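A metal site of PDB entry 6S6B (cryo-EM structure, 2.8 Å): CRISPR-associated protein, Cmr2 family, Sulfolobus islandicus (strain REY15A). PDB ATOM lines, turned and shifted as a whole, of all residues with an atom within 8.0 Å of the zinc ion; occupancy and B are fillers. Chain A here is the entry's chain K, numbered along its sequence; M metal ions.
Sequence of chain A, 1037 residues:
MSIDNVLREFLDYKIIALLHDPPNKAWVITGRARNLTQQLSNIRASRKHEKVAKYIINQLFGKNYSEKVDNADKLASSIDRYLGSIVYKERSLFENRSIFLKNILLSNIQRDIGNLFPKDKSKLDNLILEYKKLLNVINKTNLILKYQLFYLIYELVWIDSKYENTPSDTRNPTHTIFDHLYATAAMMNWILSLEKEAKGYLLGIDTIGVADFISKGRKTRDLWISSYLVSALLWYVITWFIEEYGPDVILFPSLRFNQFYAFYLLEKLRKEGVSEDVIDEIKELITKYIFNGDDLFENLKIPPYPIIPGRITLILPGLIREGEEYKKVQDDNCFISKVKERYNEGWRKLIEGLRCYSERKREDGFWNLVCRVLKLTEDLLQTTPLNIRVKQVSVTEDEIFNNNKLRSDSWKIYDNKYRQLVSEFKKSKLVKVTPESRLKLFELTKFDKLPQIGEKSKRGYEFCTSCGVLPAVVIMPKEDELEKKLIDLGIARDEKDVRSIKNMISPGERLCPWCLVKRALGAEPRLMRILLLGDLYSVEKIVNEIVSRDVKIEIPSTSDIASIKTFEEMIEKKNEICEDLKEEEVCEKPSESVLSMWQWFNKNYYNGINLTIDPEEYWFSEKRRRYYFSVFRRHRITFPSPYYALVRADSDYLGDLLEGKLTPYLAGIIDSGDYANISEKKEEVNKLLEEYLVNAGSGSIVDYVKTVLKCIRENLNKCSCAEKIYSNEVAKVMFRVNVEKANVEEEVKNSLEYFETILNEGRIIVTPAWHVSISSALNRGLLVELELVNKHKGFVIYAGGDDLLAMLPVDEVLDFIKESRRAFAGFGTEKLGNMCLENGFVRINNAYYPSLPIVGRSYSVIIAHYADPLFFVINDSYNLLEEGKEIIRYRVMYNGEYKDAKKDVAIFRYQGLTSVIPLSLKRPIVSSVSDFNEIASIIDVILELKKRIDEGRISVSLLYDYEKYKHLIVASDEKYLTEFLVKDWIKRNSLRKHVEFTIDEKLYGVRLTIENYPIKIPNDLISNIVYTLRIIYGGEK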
ATOM      1  N   LYS A 216      -8.859  16.343 -15.309  1.00  0.00           N
ATOM      2  CA  LYS A 216      -8.474  16.873 -16.614  1.00  0.00           C
ATOM      3  C   LYS A 216      -9.736  17.070 -17.434  1.00  0.00           C
ATOM      4  O   LYS A 216     -10.216  16.159 -18.108  1.00  0.00           O
ATOM      5  CB  LYS A 216      -7.493  15.934 -17.304  1.00  0.00           C
ATOM      6  CG  LYS A 216      -6.135  15.902 -16.650  1.00  0.00           C
ATOM      7  CD  LYS A 216      -5.358  14.673 -17.078  1.00  0.00           C
ATOM      8  CE  LYS A 216      -4.037  14.590 -16.365  1.00  0.00           C
ATOM      9  NZ  LYS A 216      -3.637  13.175 -16.120  1.00  0.00           N
ATOM     10  N   GLY A 217     -10.291  18.287 -17.372  1.00  0.00           N
ATOM     11  CA  GLY A 217     -11.468  18.626 -18.142  1.00  0.00           C
ATOM     12  C   GLY A 217     -11.940  20.033 -17.893  1.00  0.00           C
ATOM     13  O   GLY A 217     -11.986  20.489 -16.752  1.00  0.00           O
ATOM     14  N   GLU A 436       0.943  10.067 -19.078  1.00  0.00           N
ATOM     15  CA  GLU A 436       1.487  10.864 -20.169  1.00  0.00           C
ATOM     16  C   GLU A 436       2.923  10.501 -20.481  1.00  0.00           C
ATOM     17  O   GLU A 436       3.408  10.791 -21.584  1.00  0.00           O
ATOM     18  CB  GLU A 436       1.418  12.353 -19.825  1.00  0.00           C
ATOM     19  CG  GLU A 436       0.017  12.924 -19.873  1.00  0.00           C
ATOM     20  CD  GLU A 436      -0.810  12.539 -18.675  1.00  0.00           C
ATOM     21  OE1 GLU A 436      -0.238  12.024 -17.693  1.00  0.00           O
ATOM     22  OE2 GLU A 436      -2.041  12.734 -18.714  1.00  0.00           O
ATOM     23  N   PHE A 463      -0.007  23.904 -25.425  1.00  0.00           N
ATOM     24  CA  PHE A 463      -0.558  22.883 -24.525  1.00  0.00           C
ATOM     25  C   PHE A 463      -2.073  22.827 -24.484  1.00  0.00           C
ATOM     26  O   PHE A 463      -2.753  23.835 -24.689  1.00  0.00           O
ATOM     27  CB  PHE A 463      -0.090  23.124 -23.079  1.00  0.00           C
ATOM     28  CG  PHE A 463       1.383  23.096 -22.894  1.00  0.00           C
ATOM     29  CD1 PHE A 463       2.084  21.922 -23.034  1.00  0.00           C
ATOM     30  CD2 PHE A 463       2.058  24.235 -22.527  1.00  0.00           C
ATOM     31  CE1 PHE A 463       3.439  21.897 -22.845  1.00  0.00           C
ATOM     32  CE2 PHE A 463       3.410  24.217 -22.331  1.00  0.00           C
ATOM     33  CZ  PHE A 463       4.102  23.044 -22.493  1.00  0.00           C
ATOM     34  N   CYS A 464      -2.618  21.635 -24.223  1.00  0.00           N
ATOM     35  CA  CYS A 464      -4.056  21.468 -24.079  1.00  0.00           C
ATOM     36  C   CYS A 464      -4.587  22.318 -22.937  1.00  0.00           C
ATOM     37  O   CYS A 464      -3.874  22.616 -21.976  1.00  0.00           O
ATOM     38  CB  CYS A 464      -4.381  19.997 -23.836  1.00  0.00           C
ATOM     39  SG  CYS A 464      -6.110  19.618 -23.530  1.00  0.00           S
ATOM     40  N   THR A 465      -5.850  22.726 -23.051  1.00  0.00           N
ATOM     41  CA  THR A 465      -6.482  23.513 -21.997  1.00  0.00           C
ATOM     42  C   THR A 465      -7.151  22.652 -20.937  1.00  0.00           C
ATOM     43  O   THR A 465      -7.434  23.152 -19.848  1.00  0.00           O
ATOM     44  CB  THR A 465      -7.528  24.461 -22.582  1.00  0.00           C
ATOM     45  OG1 THR A 465      -8.349  23.757 -23.518  1.00  0.00           O
ATOM     46  CG2 THR A 465      -6.847  25.624 -23.279  1.00  0.00           C
ATOM     47  N   SER A 466      -7.410  21.385 -21.230  1.00  0.00           N
ATOM     48  CA  SER A 466      -7.952  20.478 -20.235  1.00  0.00           C
ATOM     49  C   SER A 466      -6.829  19.819 -19.437  1.00  0.00           C
ATOM     50  O   SER A 466      -6.750  19.983 -18.214  1.00  0.00           O
ATOM     51  CB  SER A 466      -8.842  19.435 -20.900  1.00  0.00           C
ATOM     52  OG  SER A 466      -9.951  20.036 -21.541  1.00  0.00           O
ATOM     53  N   CYS A 467      -5.961  19.068 -20.112  1.00  0.00           N
ATOM     54  CA  CYS A 467      -4.807  18.488 -19.441  1.00  0.00           C
ATOM     55  C   CYS A 467      -3.870  19.561 -18.904  1.00  0.00           C
ATOM     56  O   CYS A 467      -3.676  19.704 -17.698  1.00  0.00           O
ATOM     57  CB  CYS A 467      -4.045  17.565 -20.386  1.00  0.00           C
ATOM     58  SG  CYS A 467      -4.837  15.985 -20.740  1.00  0.00           S
ATOM     59  N   GLY A 468      -3.295  20.340 -19.813  1.00  0.00           N
ATOM     60  CA  GLY A 468      -2.162  21.168 -19.491  1.00  0.00           C
ATOM     61  C   GLY A 468      -0.817  20.526 -19.775  1.00  0.00           C
ATOM     62  O   GLY A 468       0.175  21.240 -19.939  1.00  0.00           O
ATOM     63  N   VAL A 469      -0.759  19.211 -19.860  1.00  0.00           N
ATOM     64  CA  VAL A 469       0.510  18.535 -20.076  1.00  0.00           C
ATOM     65  C   VAL A 469       0.767  18.270 -21.554  1.00  0.00           C
ATOM     66  O   VAL A 469       1.849  18.578 -22.069  1.00  0.00           O
ATOM     67  CB  VAL A 469       0.566  17.233 -19.235  1.00  0.00           C
ATOM     68  CG1 VAL A 469       0.631  17.581 -17.767  1.00  0.00           C
ATOM     69  CG2 VAL A 469      -0.659  16.388 -19.483  1.00  0.00           C
ATOM     70  N   LEU A 470      -0.196  17.724 -22.275  1.00  0.00           N
ATOM     71  CA  LEU A 470       0.052  17.355 -23.651  1.00  0.00           C
ATOM     72  C   LEU A 470      -0.143  18.551 -24.578  1.00  0.00           C
ATOM     73  O   LEU A 470      -0.931  19.448 -24.282  1.00  0.00           O
ATOM     74  CB  LEU A 470      -0.872  16.233 -24.076  1.00  0.00           C
ATOM     75  CG  LEU A 470      -0.776  14.967 -23.243  1.00  0.00           C
ATOM     76  CD1 LEU A 470      -1.607  13.875 -23.870  1.00  0.00           C
ATOM     77  CD2 LEU A 470       0.664  14.540 -23.120  1.00  0.00           C
ATOM     78  N   PRO A 471       0.565  18.584 -25.708  1.00  0.00           N
ATOM     79  CA  PRO A 471       0.295  19.616 -26.703  1.00  0.00           C
ATOM     80  C   PRO A 471      -1.075  19.414 -27.313  1.00  0.00           C
ATOM     81  O   PRO A 471      -1.663  18.337 -27.273  1.00  0.00           O
ATOM     82  CB  PRO A 471       1.399  19.402 -27.741  1.00  0.00           C
ATOM     83  CG  PRO A 471       2.393  18.502 -27.108  1.00  0.00           C
ATOM     84  CD  PRO A 471       1.641  17.676 -26.130  1.00  0.00           C
ATOM     85  N   ALA A 472      -1.594  20.492 -27.897  1.00  0.00           N
ATOM     86  CA  ALA A 472      -2.937  20.444 -28.449  1.00  0.00           C
ATOM     87  C   ALA A 472      -2.904  20.091 -29.929  1.00  0.00           C
ATOM     88  O   ALA A 472      -1.965  20.434 -30.651  1.00  0.00           O
ATOM     89  CB  ALA A 472      -3.664  21.767 -28.255  1.00  0.00           C
ATOM     90  N   ARG A 510      -8.093  24.888 -26.670  1.00  0.00           N
ATOM     91  CA  ARG A 510      -7.185  23.933 -27.278  1.00  0.00           C
ATOM     92  C   ARG A 510      -7.438  22.547 -26.696  1.00  0.00           C
ATOM     93  O   ARG A 510      -7.800  22.408 -25.535  1.00  0.00           O
ATOM     94  CB  ARG A 510      -5.734  24.336 -27.031  1.00  0.00           C
ATOM     95  CG  ARG A 510      -5.340  25.637 -27.672  1.00  0.00           C
ATOM     96  CD  ARG A 510      -5.378  26.760 -26.668  1.00  0.00           C
ATOM     97  NE  ARG A 510      -4.689  27.936 -27.166  1.00  0.00           N
ATOM     98  CZ  ARG A 510      -5.278  28.899 -27.859  1.00  0.00           C
ATOM     99  NH1 ARG A 510      -4.575  29.939 -28.270  1.00  0.00           N
ATOM    100  NH2 ARG A 510      -6.574  28.830 -28.119  1.00  0.00           N
ATOM    101  N   LEU A 511      -7.239  21.520 -27.525  1.00  0.00           N
ATOM    102  CA  LEU A 511      -7.536  20.155 -27.120  1.00  0.00           C
ATOM    103  C   LEU A 511      -6.447  19.215 -27.594  1.00  0.00           C
ATOM    104  O   LEU A 511      -5.976  19.314 -28.721  1.00  0.00           O
ATOM    105  CB  LEU A 511      -8.893  19.704 -27.654  1.00  0.00           C
ATOM    106  CG  LEU A 511     -10.092  20.144 -26.817  1.00  0.00           C
ATOM    107  CD1 LEU A 511     -11.372  19.540 -27.344  1.00  0.00           C
ATOM    108  CD2 LEU A 511      -9.874  19.757 -25.378  1.00  0.00           C
ATOM    109  N   CYS A 512      -6.065  18.300 -26.716  1.00  0.00           N
ATOM    110  CA  CYS A 512      -5.125  17.226 -27.039  1.00  0.00           C
ATOM    111  C   CYS A 512      -5.896  16.013 -27.543  1.00  0.00           C
ATOM    112  O   CYS A 512      -7.115  15.953 -27.420  1.00  0.00           O
ATOM    113  CB  CYS A 512      -4.291  16.897 -25.813  1.00  0.00           C
ATOM    114  SG  CYS A 512      -5.093  15.858 -24.590  1.00  0.00           S
ATOM    115  N   PRO A 513      -5.203  15.035 -28.131  1.00  0.00           N
ATOM    116  CA  PRO A 513      -5.932  13.852 -28.634  1.00  0.00           C
ATOM    117  C   PRO A 513      -6.714  13.126 -27.561  1.00  0.00           C
ATOM    118  O   PRO A 513      -7.833  12.690 -27.821  1.00  0.00           O
ATOM    119  CB  PRO A 513      -4.810  12.979 -29.205  1.00  0.00           C
ATOM    120  CG  PRO A 513      -3.742  13.917 -29.548  1.00  0.00           C
ATOM    121  CD  PRO A 513      -3.773  14.987 -28.510  1.00  0.00           C
ATOM    122  N   TRP A 514      -6.150  12.985 -26.361  1.00  0.00           N
ATOM    123  CA  TRP A 514      -6.850  12.295 -25.293  1.00  0.00           C
ATOM    124  C   TRP A 514      -8.087  13.063 -24.863  1.00  0.00           C
ATOM    125  O   TRP A 514      -9.160  12.476 -24.662  1.00  0.00           O
ATOM    126  CB  TRP A 514      -5.917  12.080 -24.106  1.00  0.00           C
ATOM    127  CG  TRP A 514      -5.007  10.924 -24.281  1.00  0.00           C
ATOM    128  CD1 TRP A 514      -5.066   9.976 -25.245  1.00  0.00           C
ATOM    129  CD2 TRP A 514      -3.894  10.583 -23.459  1.00  0.00           C
ATOM    130  NE1 TRP A 514      -4.058   9.066 -25.081  1.00  0.00           N
ATOM    131  CE2 TRP A 514      -3.328   9.417 -23.981  1.00  0.00           C
ATOM    132  CE3 TRP A 514      -3.320  11.150 -22.315  1.00  0.00           C
ATOM    133  CZ2 TRP A 514      -2.214   8.810 -23.410  1.00  0.00           C
ATOM    134  CZ3 TRP A 514      -2.219  10.550 -21.760  1.00  0.00           C
ATOM    135  CH2 TRP A 514      -1.677   9.396 -22.307  1.00  0.00           C
ATOM    136  N   CYS A 515      -7.967  14.380 -24.729  1.00  0.00           N
ATOM    137  CA  CYS A 515      -9.081  15.180 -24.228  1.00  0.00           C
ATOM    138  C   CYS A 515     -10.198  15.296 -25.256  1.00  0.00           C
ATOM    139  O   CYS A 515     -11.372  15.345 -24.884  1.00  0.00           O
ATOM    140  CB  CYS A 515      -8.600  16.555 -23.828  1.00  0.00           C
ATOM    141  SG  CYS A 515      -7.682  16.547 -22.293  1.00  0.00           S
ATOM    142  N   LEU A 516      -9.858  15.336 -26.537  1.00  0.00           N
ATOM    143  CA  LEU A 516     -10.911  15.333 -27.555  1.00  0.00           C
ATOM    144  C   LEU A 516     -11.680  14.023 -27.521  1.00  0.00           C
ATOM    145  O   LEU A 516     -12.901  14.008 -27.745  1.00  0.00           O
ATOM    146  CB  LEU A 516     -10.311  15.575 -28.936  1.00  0.00           C
ATOM    147  CG  LEU A 516     -11.372  15.719 -30.019  1.00  0.00           C
ATOM    148  CD1 LEU A 516     -11.049  16.868 -30.935  1.00  0.00           C
ATOM    149  CD2 LEU A 516     -11.504  14.427 -30.805  1.00  0.00           C
ATOM    150  N   LYS A 518     -12.249  12.492 -24.825  1.00  0.00           N
ATOM    151  CA  LYS A 518     -13.171  12.756 -23.728  1.00  0.00           C
ATOM    152  C   LYS A 518     -14.337  13.609 -24.192  1.00  0.00           C
ATOM    153  O   LYS A 518     -15.475  13.406 -23.763  1.00  0.00           O
ATOM    154  CB  LYS A 518     -12.445  13.432 -22.575  1.00  0.00           C
ATOM    155  CG  LYS A 518     -11.487  12.553 -21.790  1.00  0.00           C
ATOM    156  CD  LYS A 518     -10.891  13.354 -20.654  1.00  0.00           C
ATOM    157  CE  LYS A 518      -9.660  12.689 -20.089  1.00  0.00           C
ATOM    158  NZ  LYS A 518      -9.125  13.449 -18.918  1.00  0.00           N
HETATM  159 ZN    ZN M   1      -5.522  17.366 -22.737  1.00  0.00          ZN
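The zinc ion is bound by SG of Cys 515 (2.4 Å), SG of Cys 512 (2.4 Å), SG of Cys 464 (2.5 Å) and SG of Cys 467 (2.5 Å).
The zinc ion has four donor atoms within binding distance.
The side-chain sulfur of Cys 512 sits close to the backbone NH of Trp 514, at 3.5 Å.
The side-chain sulfur of Cys 464 lies close to the backbone NH of Ser 466, at 3.2 Å.
N of Cys 464 sits at hydrogen-bond distance from O of Leu 470, 2.8 Å away.
Of the 21 residues printed, 4 come within 4 Å of the zinc ion.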
